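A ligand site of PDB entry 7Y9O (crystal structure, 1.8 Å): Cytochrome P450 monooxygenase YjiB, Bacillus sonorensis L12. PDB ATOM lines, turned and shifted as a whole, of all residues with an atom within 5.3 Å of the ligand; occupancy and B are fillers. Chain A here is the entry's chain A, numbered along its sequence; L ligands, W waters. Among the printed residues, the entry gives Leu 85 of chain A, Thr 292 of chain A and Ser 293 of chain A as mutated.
The guanidinium group (NH1) of Arg 96 lies within salt-bridge range of an oxygen (O4) of the ligand, 2.9 Å away.
NE2 of His 92 is in hydrogen-bond range of O4 of the ligand, 2.8 Å away.
NH2 of Arg 294 lies within salt-bridge range of O2 of the ligand (2.8 Å).
OG1 of Thr 292 lies within hydrogen-bond range of O1 of the ligand.
A ring nitrogen (ND1) of His 350 lies within hydrogen-bond range of an oxygen (O3) of the ligand (2.8 Å).
An iron atom (FE1) of the ligand is bound by the side-chain sulfur of Cys 352.
NE2 of His 92 lies within hydrogen-bond range of ND1 of His 350, at 3.3 Å.
N of Gly 354 sits close to SG of Cys 352, 3.1 Å away.
The side-chain hydroxyl (OG1) of Thr 247 sits at hydrogen-bond distance from the side-chain carboxylate (OE1) of Glu 361, 2.8 Å away.
The backbone NH (N) of Cys 352 is in hydrogen-bond range of the backbone carbonyl oxygen (O) of Phe 345.
A ring nitrogen (NE2) of His 350 sits close to the side-chain amide oxygen of Asn 69 (3.4 Å).
The side-chain amide nitrogen of Asn 69 sits at hydrogen-bond distance from the backbone carbonyl oxygen of Leu 85 (2.8 Å).
The guanidinium group (NH1) of Arg 96 sits at hydrogen-bond distance from the backbone carbonyl oxygen (O) of Phe 351 (2.7 Å).
The backbone NH of Ala 355 lies close to the side-chain sulfur of Cys 352 (3.4 Å).
The side-chain sulfur (SD) of Met 84 sits close to an oxygen (O4) of the ligand.
Merely in contact with the ligand: Thr 246 (3.0 Å), Ala 358 (3.4 Å), Phe 345 (3.4 Å), Gly 346 (3.4 Å), Gly 344 (3.5 Å), Thr 247 (3.5 Å), Leu 317 (3.5 Å), Leu 85 (3.5 Å), Gly 354 (3.5 Å), Gly 243 (3.7 Å), Leu 238 (3.7 Å), Ala 242 (3.7 Å), Pro 288 (3.7 Å), Asn 69 (3.8 Å), Ile 349 (3.8 Å), Leu 357 (3.8 Å), Leu 250 (3.8 Å), Phe 103 (3.9 Å), Leu 353 (3.9 Å) and Ala 289 (3.97 Å).
27 residues have an atom within 4 Å of the ligand: Asn 69, Met 84, Leu 85, His 92, Arg 96, Phe 103, Leu 238, Ala 242, Gly 243, Thr 246, Thr 247, Leu 250, Pro 288, Ala 289, Thr 292, Arg 294, Leu 317, Gly 344, Phe 345, Gly 346, Ile 349, His 350, Cys 352, Leu 353, Gly 354, Leu 357 and Ala 358.
The nearest printed residue that does not touch the ligand is Ile 147 (4.04 Å).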
ATOM      1  N   ILE A  61      -0.199  19.383  17.631  1.00  0.00           N
ATOM      2  CA  ILE A  61      -0.056  17.988  17.088  1.00  0.00           C
ATOM      3  C   ILE A  61      -1.040  17.001  17.760  1.00  0.00           C
ATOM      4  O   ILE A  61      -1.251  15.931  17.191  1.00  0.00           O
ATOM      5  CB  ILE A  61       1.394  17.468  17.173  1.00  0.00           C
ATOM      6  CG1 ILE A  61       1.863  17.210  18.616  1.00  0.00           C
ATOM      7  CG2 ILE A  61       2.271  18.432  16.414  1.00  0.00           C
ATOM      8  CD1 ILE A  61       3.327  16.867  18.764  1.00  0.00           C
ATOM      9  N   ASN A  69      -5.358  16.387  10.545  1.00  0.00           N
ATOM     10  CA  ASN A  69      -4.274  15.920   9.650  1.00  0.00           C
ATOM     11  C   ASN A  69      -4.647  15.963   8.167  1.00  0.00           C
ATOM     12  O   ASN A  69      -3.796  15.550   7.376  1.00  0.00           O
ATOM     13  CB  ASN A  69      -3.830  14.507  10.005  1.00  0.00           C
ATOM     14  CG  ASN A  69      -2.825  14.591  11.124  1.00  0.00           C
ATOM     15  OD1 ASN A  69      -3.105  15.215  12.142  1.00  0.00           O
ATOM     16  ND2 ASN A  69      -1.684  13.951  10.927  1.00  0.00           N
ATOM     17  N   MET A  84      -2.103   7.037   6.502  1.00  0.00           N
ATOM     18  CA  MET A  84      -2.649   7.351   7.852  1.00  0.00           C
ATOM     19  C   MET A  84      -2.172   8.759   8.266  1.00  0.00           C
ATOM     20  O   MET A  84      -2.911   9.519   8.967  1.00  0.00           O
ATOM     21  CB  MET A  84      -2.220   6.310   8.901  1.00  0.00           C
ATOM     22  CG  MET A  84      -0.743   6.346   9.247  1.00  0.00           C
ATOM     23  SD  MET A  84      -0.305   5.028  10.381  1.00  0.00           S
ATOM     24  CE  MET A  84      -0.275   3.644   9.241  1.00  0.00           C
ATOM     25  N   LEU A  85      -1.045   9.198   7.722  1.00  0.00           N
ATOM     26  CA  LEU A  85      -0.451  10.516   8.081  1.00  0.00           C
ATOM     27  C   LEU A  85      -1.440  11.628   7.725  1.00  0.00           C
ATOM     28  O   LEU A  85      -1.376  12.658   8.415  1.00  0.00           O
ATOM     29  CB  LEU A  85       0.825  10.655   7.254  1.00  0.00           C
ATOM     30  CG  LEU A  85       1.993  11.446   7.826  1.00  0.00           C
ATOM     31  CD1 LEU A  85       2.229  11.136   9.274  1.00  0.00           C
ATOM     32  CD2 LEU A  85       3.242  11.164   7.001  1.00  0.00           C
ATOM     33  N   HIS A  92      -8.675   6.965  10.108  1.00  0.00           N
ATOM     34  CA  HIS A  92      -7.289   6.839  10.635  1.00  0.00           C
ATOM     35  C   HIS A  92      -7.146   5.623  11.543  1.00  0.00           C
ATOM     36  O   HIS A  92      -6.167   4.880  11.390  1.00  0.00           O
ATOM     37  CB  HIS A  92      -6.872   8.096  11.399  1.00  0.00           C
ATOM     38  CG  HIS A  92      -5.552   7.955  12.085  1.00  0.00           C
ATOM     39  ND1 HIS A  92      -5.442   7.620  13.418  1.00  0.00           N
ATOM     40  CD2 HIS A  92      -4.291   8.066  11.613  1.00  0.00           C
ATOM     41  CE1 HIS A  92      -4.170   7.553  13.746  1.00  0.00           C
ATOM     42  NE2 HIS A  92      -3.441   7.811  12.662  1.00  0.00           N
ATOM     43  N   ARG A  96      -4.406   2.577  10.718  1.00  0.00           N
ATOM     44  CA  ARG A  96      -3.273   2.399  11.668  1.00  0.00           C
ATOM     45  C   ARG A  96      -3.363   1.009  12.326  1.00  0.00           C
ATOM     46  O   ARG A  96      -2.302   0.344  12.458  1.00  0.00           O
ATOM     47  CB  ARG A  96      -3.262   3.537  12.672  1.00  0.00           C
ATOM     48  CG  ARG A  96      -2.062   3.436  13.597  1.00  0.00           C
ATOM     49  CD  ARG A  96      -1.747   4.671  14.388  1.00  0.00           C
ATOM     50  NE  ARG A  96      -0.682   4.372  15.341  1.00  0.00           N
ATOM     51  CZ  ARG A  96       0.326   5.189  15.652  1.00  0.00           C
ATOM     52  NH1 ARG A  96       0.436   6.364  15.086  1.00  0.00           N
ATOM     53  NH2 ARG A  96       1.217   4.803  16.565  1.00  0.00           N
ATOM     54  N   PHE A 103       4.268  -3.296  14.853  1.00  0.00           N
ATOM     55  CA  PHE A 103       5.325  -2.288  15.111  1.00  0.00           C
ATOM     56  C   PHE A 103       5.531  -2.109  16.616  1.00  0.00           C
ATOM     57  O   PHE A 103       6.273  -1.163  16.968  1.00  0.00           O
ATOM     58  CB  PHE A 103       4.962  -0.976  14.420  1.00  0.00           C
ATOM     59  CG  PHE A 103       5.328  -0.996  12.965  1.00  0.00           C
ATOM     60  CD1 PHE A 103       6.631  -0.745  12.568  1.00  0.00           C
ATOM     61  CD2 PHE A 103       4.398  -1.348  11.991  1.00  0.00           C
ATOM     62  CE1 PHE A 103       6.989  -0.790  11.241  1.00  0.00           C
ATOM     63  CE2 PHE A 103       4.775  -1.415  10.663  1.00  0.00           C
ATOM     64  CZ  PHE A 103       6.070  -1.124  10.295  1.00  0.00           C
ATOM     65  N   ILE A 147      14.277  -2.153   6.978  1.00  0.00           N
ATOM     66  CA  ILE A 147      12.891  -1.818   6.529  1.00  0.00           C
ATOM     67  C   ILE A 147      12.526  -2.658   5.295  1.00  0.00           C
ATOM     68  O   ILE A 147      11.381  -3.150   5.224  1.00  0.00           O
ATOM     69  CB  ILE A 147      12.637  -0.313   6.320  1.00  0.00           C
ATOM     70  CG1 ILE A 147      11.118  -0.095   6.352  1.00  0.00           C
ATOM     71  CG2 ILE A 147      13.279   0.196   5.035  1.00  0.00           C
ATOM     72  CD1 ILE A 147      10.440  -0.443   7.681  1.00  0.00           C
ATOM     73  N   LEU A 238       5.087   5.020   2.337  1.00  0.00           N
ATOM     74  CA  LEU A 238       5.236   5.686   3.646  1.00  0.00           C
ATOM     75  C   LEU A 238       6.158   4.868   4.557  1.00  0.00           C
ATOM     76  O   LEU A 238       7.094   5.448   5.155  1.00  0.00           O
ATOM     77  CB  LEU A 238       3.869   5.891   4.279  1.00  0.00           C
ATOM     78  CG  LEU A 238       3.945   6.213   5.761  1.00  0.00           C
ATOM     79  CD1 LEU A 238       4.608   7.555   5.919  1.00  0.00           C
ATOM     80  CD2 LEU A 238       2.562   6.175   6.402  1.00  0.00           C
ATOM     81  N   LEU A 239       5.958   3.559   4.668  1.00  0.00           N
ATOM     82  CA  LEU A 239       6.791   2.769   5.590  1.00  0.00           C
ATOM     83  C   LEU A 239       8.230   2.698   5.046  1.00  0.00           C
ATOM     84  O   LEU A 239       9.181   2.724   5.891  1.00  0.00           O
ATOM     85  CB  LEU A 239       6.203   1.360   5.769  1.00  0.00           C
ATOM     86  CG  LEU A 239       4.817   1.313   6.425  1.00  0.00           C
ATOM     87  CD1 LEU A 239       4.295  -0.118   6.367  1.00  0.00           C
ATOM     88  CD2 LEU A 239       4.849   1.819   7.881  1.00  0.00           C
ATOM     89  N   ALA A 242       9.771   6.629   5.427  1.00  0.00           N
ATOM     90  CA  ALA A 242       9.902   6.953   6.857  1.00  0.00           C
ATOM     91  C   ALA A 242      10.925   5.990   7.509  1.00  0.00           C
ATOM     92  O   ALA A 242      11.769   6.465   8.288  1.00  0.00           O
ATOM     93  CB  ALA A 242       8.555   6.873   7.546  1.00  0.00           C
ATOM     94  N   GLY A 243      10.878   4.719   7.151  1.00  0.00           N
ATOM     95  CA  GLY A 243      11.645   3.636   7.781  1.00  0.00           C
ATOM     96  C   GLY A 243      13.128   3.839   7.644  1.00  0.00           C
ATOM     97  O   GLY A 243      13.880   3.393   8.557  1.00  0.00           O
ATOM     98  N   THR A 246      14.177   8.580   8.515  1.00  0.00           N
ATOM     99  CA  THR A 246      14.150   8.970   9.939  1.00  0.00           C
ATOM    100  C   THR A 246      15.377   8.364  10.623  1.00  0.00           C
ATOM    101  O   THR A 246      16.214   9.168  11.105  1.00  0.00           O
ATOM    102  CB  THR A 246      12.855   8.539  10.619  1.00  0.00           C
ATOM    103  OG1 THR A 246      12.791   7.113  10.539  1.00  0.00           O
ATOM    104  CG2 THR A 246      11.626   9.218  10.034  1.00  0.00           C
ATOM    105  N   THR A 247      15.487   7.050  10.655  1.00  0.00           N
ATOM    106  CA  THR A 247      16.531   6.331  11.412  1.00  0.00           C
ATOM    107  C   THR A 247      17.924   6.653  10.848  1.00  0.00           C
ATOM    108  O   THR A 247      18.845   6.787  11.673  1.00  0.00           O
ATOM    109  CB  THR A 247      16.350   4.811  11.365  1.00  0.00           C
ATOM    110  OG1 THR A 247      15.036   4.534  11.833  1.00  0.00           O
ATOM    111  CG2 THR A 247      17.407   4.122  12.199  1.00  0.00           C
ATOM    112  N   LEU A 250      18.626  10.078  12.275  1.00  0.00           N
ATOM    113  CA  LEU A 250      18.742   9.998  13.763  1.00  0.00           C
ATOM    114  C   LEU A 250      20.106   9.398  14.186  1.00  0.00           C
ATOM    115  O   LEU A 250      20.741   9.930  15.181  1.00  0.00           O
ATOM    116  CB  LEU A 250      17.588   9.244  14.394  1.00  0.00           C
ATOM    117  CG  LEU A 250      17.682   9.108  15.919  1.00  0.00           C
ATOM    118  CD1 LEU A 250      17.602  10.459  16.572  1.00  0.00           C
ATOM    119  CD2 LEU A 250      16.585   8.180  16.405  1.00  0.00           C
ATOM    120  N   VAL A 283      16.711  12.347  19.934  1.00  0.00           N
ATOM    121  CA  VAL A 283      15.337  12.639  19.392  1.00  0.00           C
ATOM    122  C   VAL A 283      14.900  14.037  19.851  1.00  0.00           C
ATOM    123  O   VAL A 283      14.349  14.798  19.056  1.00  0.00           O
ATOM    124  CB  VAL A 283      14.326  11.543  19.769  1.00  0.00           C
ATOM    125  CG1 VAL A 283      12.910  11.965  19.349  1.00  0.00           C
ATOM    126  CG2 VAL A 283      14.697  10.200  19.136  1.00  0.00           C
ATOM    127  N   ALA A 287      16.385  15.616  16.046  1.00  0.00           N
ATOM    128  CA  ALA A 287      15.492  14.610  15.439  1.00  0.00           C
ATOM    129  C   ALA A 287      15.573  14.739  13.920  1.00  0.00           C
ATOM    130  O   ALA A 287      15.835  15.817  13.411  1.00  0.00           O
ATOM    131  CB  ALA A 287      14.088  14.775  15.940  1.00  0.00           C
ATOM    132  N   PRO A 288      15.344  13.640  13.161  1.00  0.00           N
ATOM    133  CA  PRO A 288      15.235  13.729  11.715  1.00  0.00           C
ATOM    134  C   PRO A 288      13.973  14.441  11.238  1.00  0.00           C
ATOM    135  O   PRO A 288      13.949  14.800  10.070  1.00  0.00           O
ATOM    136  CB  PRO A 288      15.285  12.263  11.268  1.00  0.00           C
ATOM    137  CG  PRO A 288      14.714  11.528  12.472  1.00  0.00           C
ATOM    138  CD  PRO A 288      15.244  12.274  13.663  1.00  0.00           C
ATOM    139  N   ALA A 289      12.956  14.582  12.123  1.00  0.00           N
ATOM    140  CA  ALA A 289      11.638  15.158  11.762  1.00  0.00           C
ATOM    141  C   ALA A 289      11.409  16.436  12.550  1.00  0.00           C
ATOM    142  O   ALA A 289      10.823  16.431  13.627  1.00  0.00           O
ATOM    143  CB  ALA A 289      10.511  14.158  11.974  1.00  0.00           C
ATOM    144  N   THR A 292       5.836  18.950  11.857  1.00  0.00           N
ATOM    145  CA  THR A 292       4.681  18.353  11.136  1.00  0.00           C
ATOM    146  C   THR A 292       3.672  19.459  10.943  1.00  0.00           C
ATOM    147  O   THR A 292       3.964  20.615  11.317  1.00  0.00           O
ATOM    148  CB  THR A 292       4.180  17.094  11.841  1.00  0.00           C
ATOM    149  OG1 THR A 292       3.269  16.502  10.902  1.00  0.00           O
ATOM    150  CG2 THR A 292       3.536  17.336  13.189  1.00  0.00           C
ATOM    151  N   SER A 293       2.556  19.153  10.304  1.00  0.00           N
ATOM    152  CA  SER A 293       1.586  20.186   9.919  1.00  0.00           C
ATOM    153  C   SER A 293       0.191  19.733  10.299  1.00  0.00           C
ATOM    154  O   SER A 293      -0.118  18.496  10.343  1.00  0.00           O
ATOM    155  CB  SER A 293       1.718  20.599   8.496  1.00  0.00           C
ATOM    156  OG  SER A 293       1.550  19.531   7.620  1.00  0.00           O
ATOM    157  N   ARG A 294      -0.664  20.730  10.524  1.00  0.00           N
ATOM    158  CA  ARG A 294      -2.079  20.493  10.812  1.00  0.00           C
ATOM    159  C   ARG A 294      -2.910  21.516  10.052  1.00  0.00           C
ATOM    160  O   ARG A 294      -2.336  22.556   9.548  1.00  0.00           O
ATOM    161  CB  ARG A 294      -2.337  20.613  12.304  1.00  0.00           C
ATOM    162  CG  ARG A 294      -1.639  19.576  13.171  1.00  0.00           C
ATOM    163  CD  ARG A 294      -2.259  18.198  12.997  1.00  0.00           C
ATOM    164  NE  ARG A 294      -1.692  17.201  13.862  1.00  0.00           N
ATOM    165  CZ  ARG A 294      -0.685  16.404  13.580  1.00  0.00           C
ATOM    166  NH1 ARG A 294      -0.046  16.468  12.409  1.00  0.00           N
ATOM    167  NH2 ARG A 294      -0.325  15.513  14.477  1.00  0.00           N
ATOM    168  N   LEU A 317       8.386  20.777  16.070  1.00  0.00           N
ATOM    169  CA  LEU A 317       8.819  19.803  17.091  1.00  0.00           C
ATOM    170  C   LEU A 317      10.234  20.107  17.560  1.00  0.00           C
ATOM    171  O   LEU A 317      10.472  20.019  18.794  1.00  0.00           O
ATOM    172  CB  LEU A 317       8.792  18.387  16.506  1.00  0.00           C
ATOM    173  CG  LEU A 317       7.446  17.972  15.914  1.00  0.00           C
ATOM    174  CD1 LEU A 317       7.649  16.707  15.113  1.00  0.00           C
ATOM    175  CD2 LEU A 317       6.444  17.777  17.011  1.00  0.00           C
ATOM    176  N   ILE A 343       8.712  15.713  22.672  1.00  0.00           N
ATOM    177  CA  ILE A 343       7.627  15.346  21.720  1.00  0.00           C
ATOM    178  C   ILE A 343       8.212  15.090  20.318  1.00  0.00           C
ATOM    179  O   ILE A 343       7.522  15.324  19.297  1.00  0.00           O
ATOM    180  CB  ILE A 343       6.512  16.391  21.717  1.00  0.00           C
ATOM    181  CG1 ILE A 343       7.027  17.802  21.372  1.00  0.00           C
ATOM    182  CG2 ILE A 343       5.747  16.322  23.050  1.00  0.00           C
ATOM    183  CD1 ILE A 343       5.952  18.856  21.260  1.00  0.00           C
ATOM    184  N   GLY A 344       9.425  14.551  20.267  1.00  0.00           N
ATOM    185  CA  GLY A 344      10.168  14.347  19.006  1.00  0.00           C
ATOM    186  C   GLY A 344       9.543  13.262  18.131  1.00  0.00           C
ATOM    187  O   GLY A 344       9.773  13.326  16.910  1.00  0.00           O
ATOM    188  N   PHE A 345       8.780  12.342  18.715  1.00  0.00           N
ATOM    189  CA  PHE A 345       8.000  11.270  18.025  1.00  0.00           C
ATOM    190  C   PHE A 345       6.556  11.725  17.826  1.00  0.00           C
ATOM    191  O   PHE A 345       5.722  10.921  17.400  1.00  0.00           O
ATOM    192  CB  PHE A 345       8.118   9.937  18.778  1.00  0.00           C
ATOM    193  CG  PHE A 345       9.450   9.226  18.643  1.00  0.00           C
ATOM    194  CD1 PHE A 345       9.904   8.783  17.404  1.00  0.00           C
ATOM    195  CD2 PHE A 345      10.207   8.944  19.781  1.00  0.00           C
ATOM    196  CE1 PHE A 345      11.102   8.091  17.317  1.00  0.00           C
ATOM    197  CE2 PHE A 345      11.403   8.264  19.674  1.00  0.00           C
ATOM    198  CZ  PHE A 345      11.851   7.838  18.449  1.00  0.00           C
ATOM    199  N   GLY A 346       6.240  12.972  18.180  1.00  0.00           N
ATOM    200  CA  GLY A 346       4.871  13.516  18.161  1.00  0.00           C
ATOM    201  C   GLY A 346       4.120  13.243  19.466  1.00  0.00           C
ATOM    202  O   GLY A 346       4.743  12.920  20.490  1.00  0.00           O
ATOM    203  N   ILE A 349      -2.703  10.771  18.605  1.00  0.00           N
ATOM    204  CA  ILE A 349      -3.093   9.545  17.861  1.00  0.00           C
ATOM    205  C   ILE A 349      -2.085   9.252  16.729  1.00  0.00           C
ATOM    206  O   ILE A 349      -2.074   8.106  16.276  1.00  0.00           O
ATOM    207  CB  ILE A 349      -4.564   9.617  17.402  1.00  0.00           C
ATOM    208  CG1 ILE A 349      -4.815  10.777  16.436  1.00  0.00           C
ATOM    209  CG2 ILE A 349      -5.447   9.692  18.627  1.00  0.00           C
ATOM    210  CD1 ILE A 349      -6.090  10.649  15.642  1.00  0.00           C
ATOM    211  N   HIS A 350      -1.375  10.261  16.226  1.00  0.00           N
ATOM    212  CA  HIS A 350      -0.376  10.135  15.129  1.00  0.00           C
ATOM    213  C   HIS A 350       1.030   9.896  15.698  1.00  0.00           C
ATOM    214  O   HIS A 350       1.989   9.790  14.901  1.00  0.00           O
ATOM    215  CB  HIS A 350      -0.430  11.311  14.175  1.00  0.00           C
ATOM    216  CG  HIS A 350      -1.744  11.436  13.460  1.00  0.00           C
ATOM    217  ND1 HIS A 350      -1.996  10.763  12.277  1.00  0.00           N
ATOM    218  CD2 HIS A 350      -2.853  12.153  13.754  1.00  0.00           C
ATOM    219  CE1 HIS A 350      -3.227  11.081  11.862  1.00  0.00           C
ATOM    220  NE2 HIS A 350      -3.758  11.947  12.758  1.00  0.00           N
ATOM    221  N   PHE A 351       1.135   9.655  17.010  1.00  0.00           N
ATOM    222  CA  PHE A 351       2.426   9.322  17.655  1.00  0.00           C
ATOM    223  C   PHE A 351       3.181   8.318  16.770  1.00  0.00           C
ATOM    224  O   PHE A 351       2.600   7.269  16.403  1.00  0.00           O
ATOM    225  CB  PHE A 351       2.236   8.711  19.046  1.00  0.00           C
ATOM    226  CG  PHE A 351       3.548   8.483  19.739  1.00  0.00           C
ATOM    227  CD1 PHE A 351       4.237   7.305  19.551  1.00  0.00           C
ATOM    228  CD2 PHE A 351       4.131   9.474  20.503  1.00  0.00           C
ATOM    229  CE1 PHE A 351       5.481   7.124  20.128  1.00  0.00           C
ATOM    230  CE2 PHE A 351       5.349   9.273  21.137  1.00  0.00           C
ATOM    231  CZ  PHE A 351       6.020   8.106  20.928  1.00  0.00           C
ATOM    232  N   CYS A 352       4.445   8.594  16.453  1.00  0.00           N
ATOM    233  CA  CYS A 352       5.247   7.767  15.480  1.00  0.00           C
ATOM    234  C   CYS A 352       5.030   6.263  15.683  1.00  0.00           C
ATOM    235  O   CYS A 352       5.381   5.703  16.729  1.00  0.00           O
ATOM    236  CB  CYS A 352       6.734   8.042  15.584  1.00  0.00           C
ATOM    237  SG  CYS A 352       7.713   7.099  14.412  1.00  0.00           S
ATOM    238  N   LEU A 353       4.512   5.596  14.654  1.00  0.00           N
ATOM    239  CA  LEU A 353       4.381   4.139  14.577  1.00  0.00           C
ATOM    240  C   LEU A 353       5.756   3.488  14.624  1.00  0.00           C
ATOM    241  O   LEU A 353       5.838   2.387  15.117  1.00  0.00           O
ATOM    242  CB  LEU A 353       3.680   3.819  13.253  1.00  0.00           C
ATOM    243  CG  LEU A 353       3.415   2.341  12.998  1.00  0.00           C
ATOM    244  CD1 LEU A 353       2.343   1.849  13.950  1.00  0.00           C
ATOM    245  CD2 LEU A 353       3.031   2.149  11.523  1.00  0.00           C
ATOM    246  N   GLY A 354       6.782   4.122  14.099  1.00  0.00           N
ATOM    247  CA  GLY A 354       8.113   3.493  14.021  1.00  0.00           C
ATOM    248  C   GLY A 354       8.973   3.742  15.245  1.00  0.00           C
ATOM    249  O   GLY A 354      10.164   3.320  15.216  1.00  0.00           O
ATOM    250  N   ALA A 355       8.459   4.397  16.282  1.00  0.00           N
ATOM    251  CA  ALA A 355       9.333   4.808  17.414  1.00  0.00           C
ATOM    252  C   ALA A 355      10.036   3.588  18.018  1.00  0.00           C
ATOM    253  O   ALA A 355      11.240   3.637  18.264  1.00  0.00           O
ATOM    254  CB  ALA A 355       8.578   5.598  18.456  1.00  0.00           C
ATOM    255  N   LEU A 357      10.854   0.671  16.636  1.00  0.00           N
ATOM    256  CA  LEU A 357      11.882   0.200  15.673  1.00  0.00           C
ATOM    257  C   LEU A 357      13.076   1.156  15.671  1.00  0.00           C
ATOM    258  O   LEU A 357      14.231   0.661  15.593  1.00  0.00           O
ATOM    259  CB  LEU A 357      11.285   0.084  14.266  1.00  0.00           C
ATOM    260  CG  LEU A 357      12.249  -0.345  13.150  1.00  0.00           C
ATOM    261  CD1 LEU A 357      12.975  -1.632  13.491  1.00  0.00           C
ATOM    262  CD2 LEU A 357      11.453  -0.518  11.844  1.00  0.00           C
ATOM    263  N   ALA A 358      12.779   2.460  15.592  1.00  0.00           N
ATOM    264  CA  ALA A 358      13.783   3.533  15.520  1.00  0.00           C
ATOM    265  C   ALA A 358      14.658   3.476  16.780  1.00  0.00           C
ATOM    266  O   ALA A 358      15.913   3.590  16.669  1.00  0.00           O
ATOM    267  CB  ALA A 358      13.109   4.865  15.403  1.00  0.00           C
ATOM    268  N   GLU A 361      16.870   0.203  16.463  1.00  0.00           N
ATOM    269  CA  GLU A 361      17.927   0.334  15.427  1.00  0.00           C
ATOM    270  C   GLU A 361      19.036   1.271  15.910  1.00  0.00           C
ATOM    271  O   GLU A 361      20.236   0.953  15.675  1.00  0.00           O
ATOM    272  CB  GLU A 361      17.384   0.879  14.101  1.00  0.00           C
ATOM    273  CG  GLU A 361      16.481  -0.057  13.332  1.00  0.00           C
ATOM    274  CD  GLU A 361      15.692   0.586  12.174  1.00  0.00           C
ATOM    275  OE1 GLU A 361      15.320   1.788  12.247  1.00  0.00           O
ATOM    276  OE2 GLU A 361      15.426  -0.118  11.239  1.00  0.00           O
HETATM  277  C1  LIG L   1       4.742   9.496  12.522  1.00  0.00           C
HETATM  278  C2  LIG L   1       8.926  11.148  14.015  1.00  0.00           C
HETATM  279  C3  LIG L   1      10.950   6.878  12.923  1.00  0.00           C
HETATM  280  C4  LIG L   1       6.898   5.657  10.609  1.00  0.00           C
HETATM  281  C5  LIG L   1       5.688  10.253  13.098  1.00  0.00           C
HETATM  282  C6  LIG L   1       5.420  11.504  13.747  1.00  0.00           C
HETATM  283  C7  LIG L   1       6.621  11.996  14.120  1.00  0.00           C
HETATM  284  C8  LIG L   1       7.607  11.058  13.712  1.00  0.00           C
HETATM  285  C9  LIG L   1       6.846  13.292  14.837  1.00  0.00           C
HETATM  286  C10 LIG L   1       4.112  12.205  13.973  1.00  0.00           C
HETATM  287  C11 LIG L   1       3.710  13.007  12.746  1.00  0.00           C
HETATM  288  C12 LIG L   1       2.457  13.791  12.962  1.00  0.00           C
HETATM  289  O1  LIG L   1       1.921  14.377  12.004  1.00  0.00           O
HETATM  290  O2  LIG L   1       1.935  13.923  14.078  1.00  0.00           O
HETATM  291  C13 LIG L   1       9.845  10.071  13.851  1.00  0.00           C
HETATM  292  C14 LIG L   1      11.203  10.177  14.287  1.00  0.00           C
HETATM  293  C15 LIG L   1      11.785   8.989  14.005  1.00  0.00           C
HETATM  294  C16 LIG L   1      10.730   8.143  13.385  1.00  0.00           C
HETATM  295  C17 LIG L   1      11.873  11.336  15.025  1.00  0.00           C
HETATM  296  C18 LIG L   1      13.182   8.643  14.305  1.00  0.00           C
HETATM  297  C19 LIG L   1      13.877   7.681  13.720  1.00  0.00           C
HETATM  298  C20 LIG L   1      10.048   6.172  12.153  1.00  0.00           C
HETATM  299  C21 LIG L   1      10.288   4.926  11.534  1.00  0.00           C
HETATM  300  C22 LIG L   1       9.152   4.606  10.818  1.00  0.00           C
HETATM  301  C23 LIG L   1       8.194   5.650  11.076  1.00  0.00           C
HETATM  302  C24 LIG L   1      11.596   4.142  11.605  1.00  0.00           C
HETATM  303  C25 LIG L   1       8.783   3.403  10.066  1.00  0.00           C
HETATM  304  C26 LIG L   1       9.249   2.241  10.455  1.00  0.00           C
HETATM  305  C27 LIG L   1       5.960   6.625  10.986  1.00  0.00           C
HETATM  306  C28 LIG L   1       4.514   6.547  10.590  1.00  0.00           C
HETATM  307  C29 LIG L   1       3.923   7.610  11.141  1.00  0.00           C
HETATM  308  C30 LIG L   1       4.991   8.325  11.874  1.00  0.00           C
HETATM  309  C31 LIG L   1       3.893   5.495   9.772  1.00  0.00           C
HETATM  310  C32 LIG L   1       2.450   7.992  11.036  1.00  0.00           C
HETATM  311  C33 LIG L   1       1.634   7.697  12.258  1.00  0.00           C
HETATM  312  C34 LIG L   1       0.214   8.150  12.080  1.00  0.00           C
HETATM  313  O3  LIG L   1      -0.111   9.023  11.259  1.00  0.00           O
HETATM  314  O4  LIG L   1      -0.692   7.626  12.783  1.00  0.00           O
HETATM  315  N1  LIG L   1       6.982   9.981  13.106  1.00  0.00           N
HETATM  316  N2  LIG L   1       9.648   8.913  13.281  1.00  0.00           N
HETATM  317  N3  LIG L   1       8.755   6.585  11.862  1.00  0.00           N
HETATM  318  N4  LIG L   1       6.159   7.717  11.697  1.00  0.00           N
HETATM  319 FE1  LIG L   1       7.798   8.284  12.530  1.00  0.00          FE
HETATM  320  O   HOH W   1       1.771  13.625  16.890  1.00  0.00           O
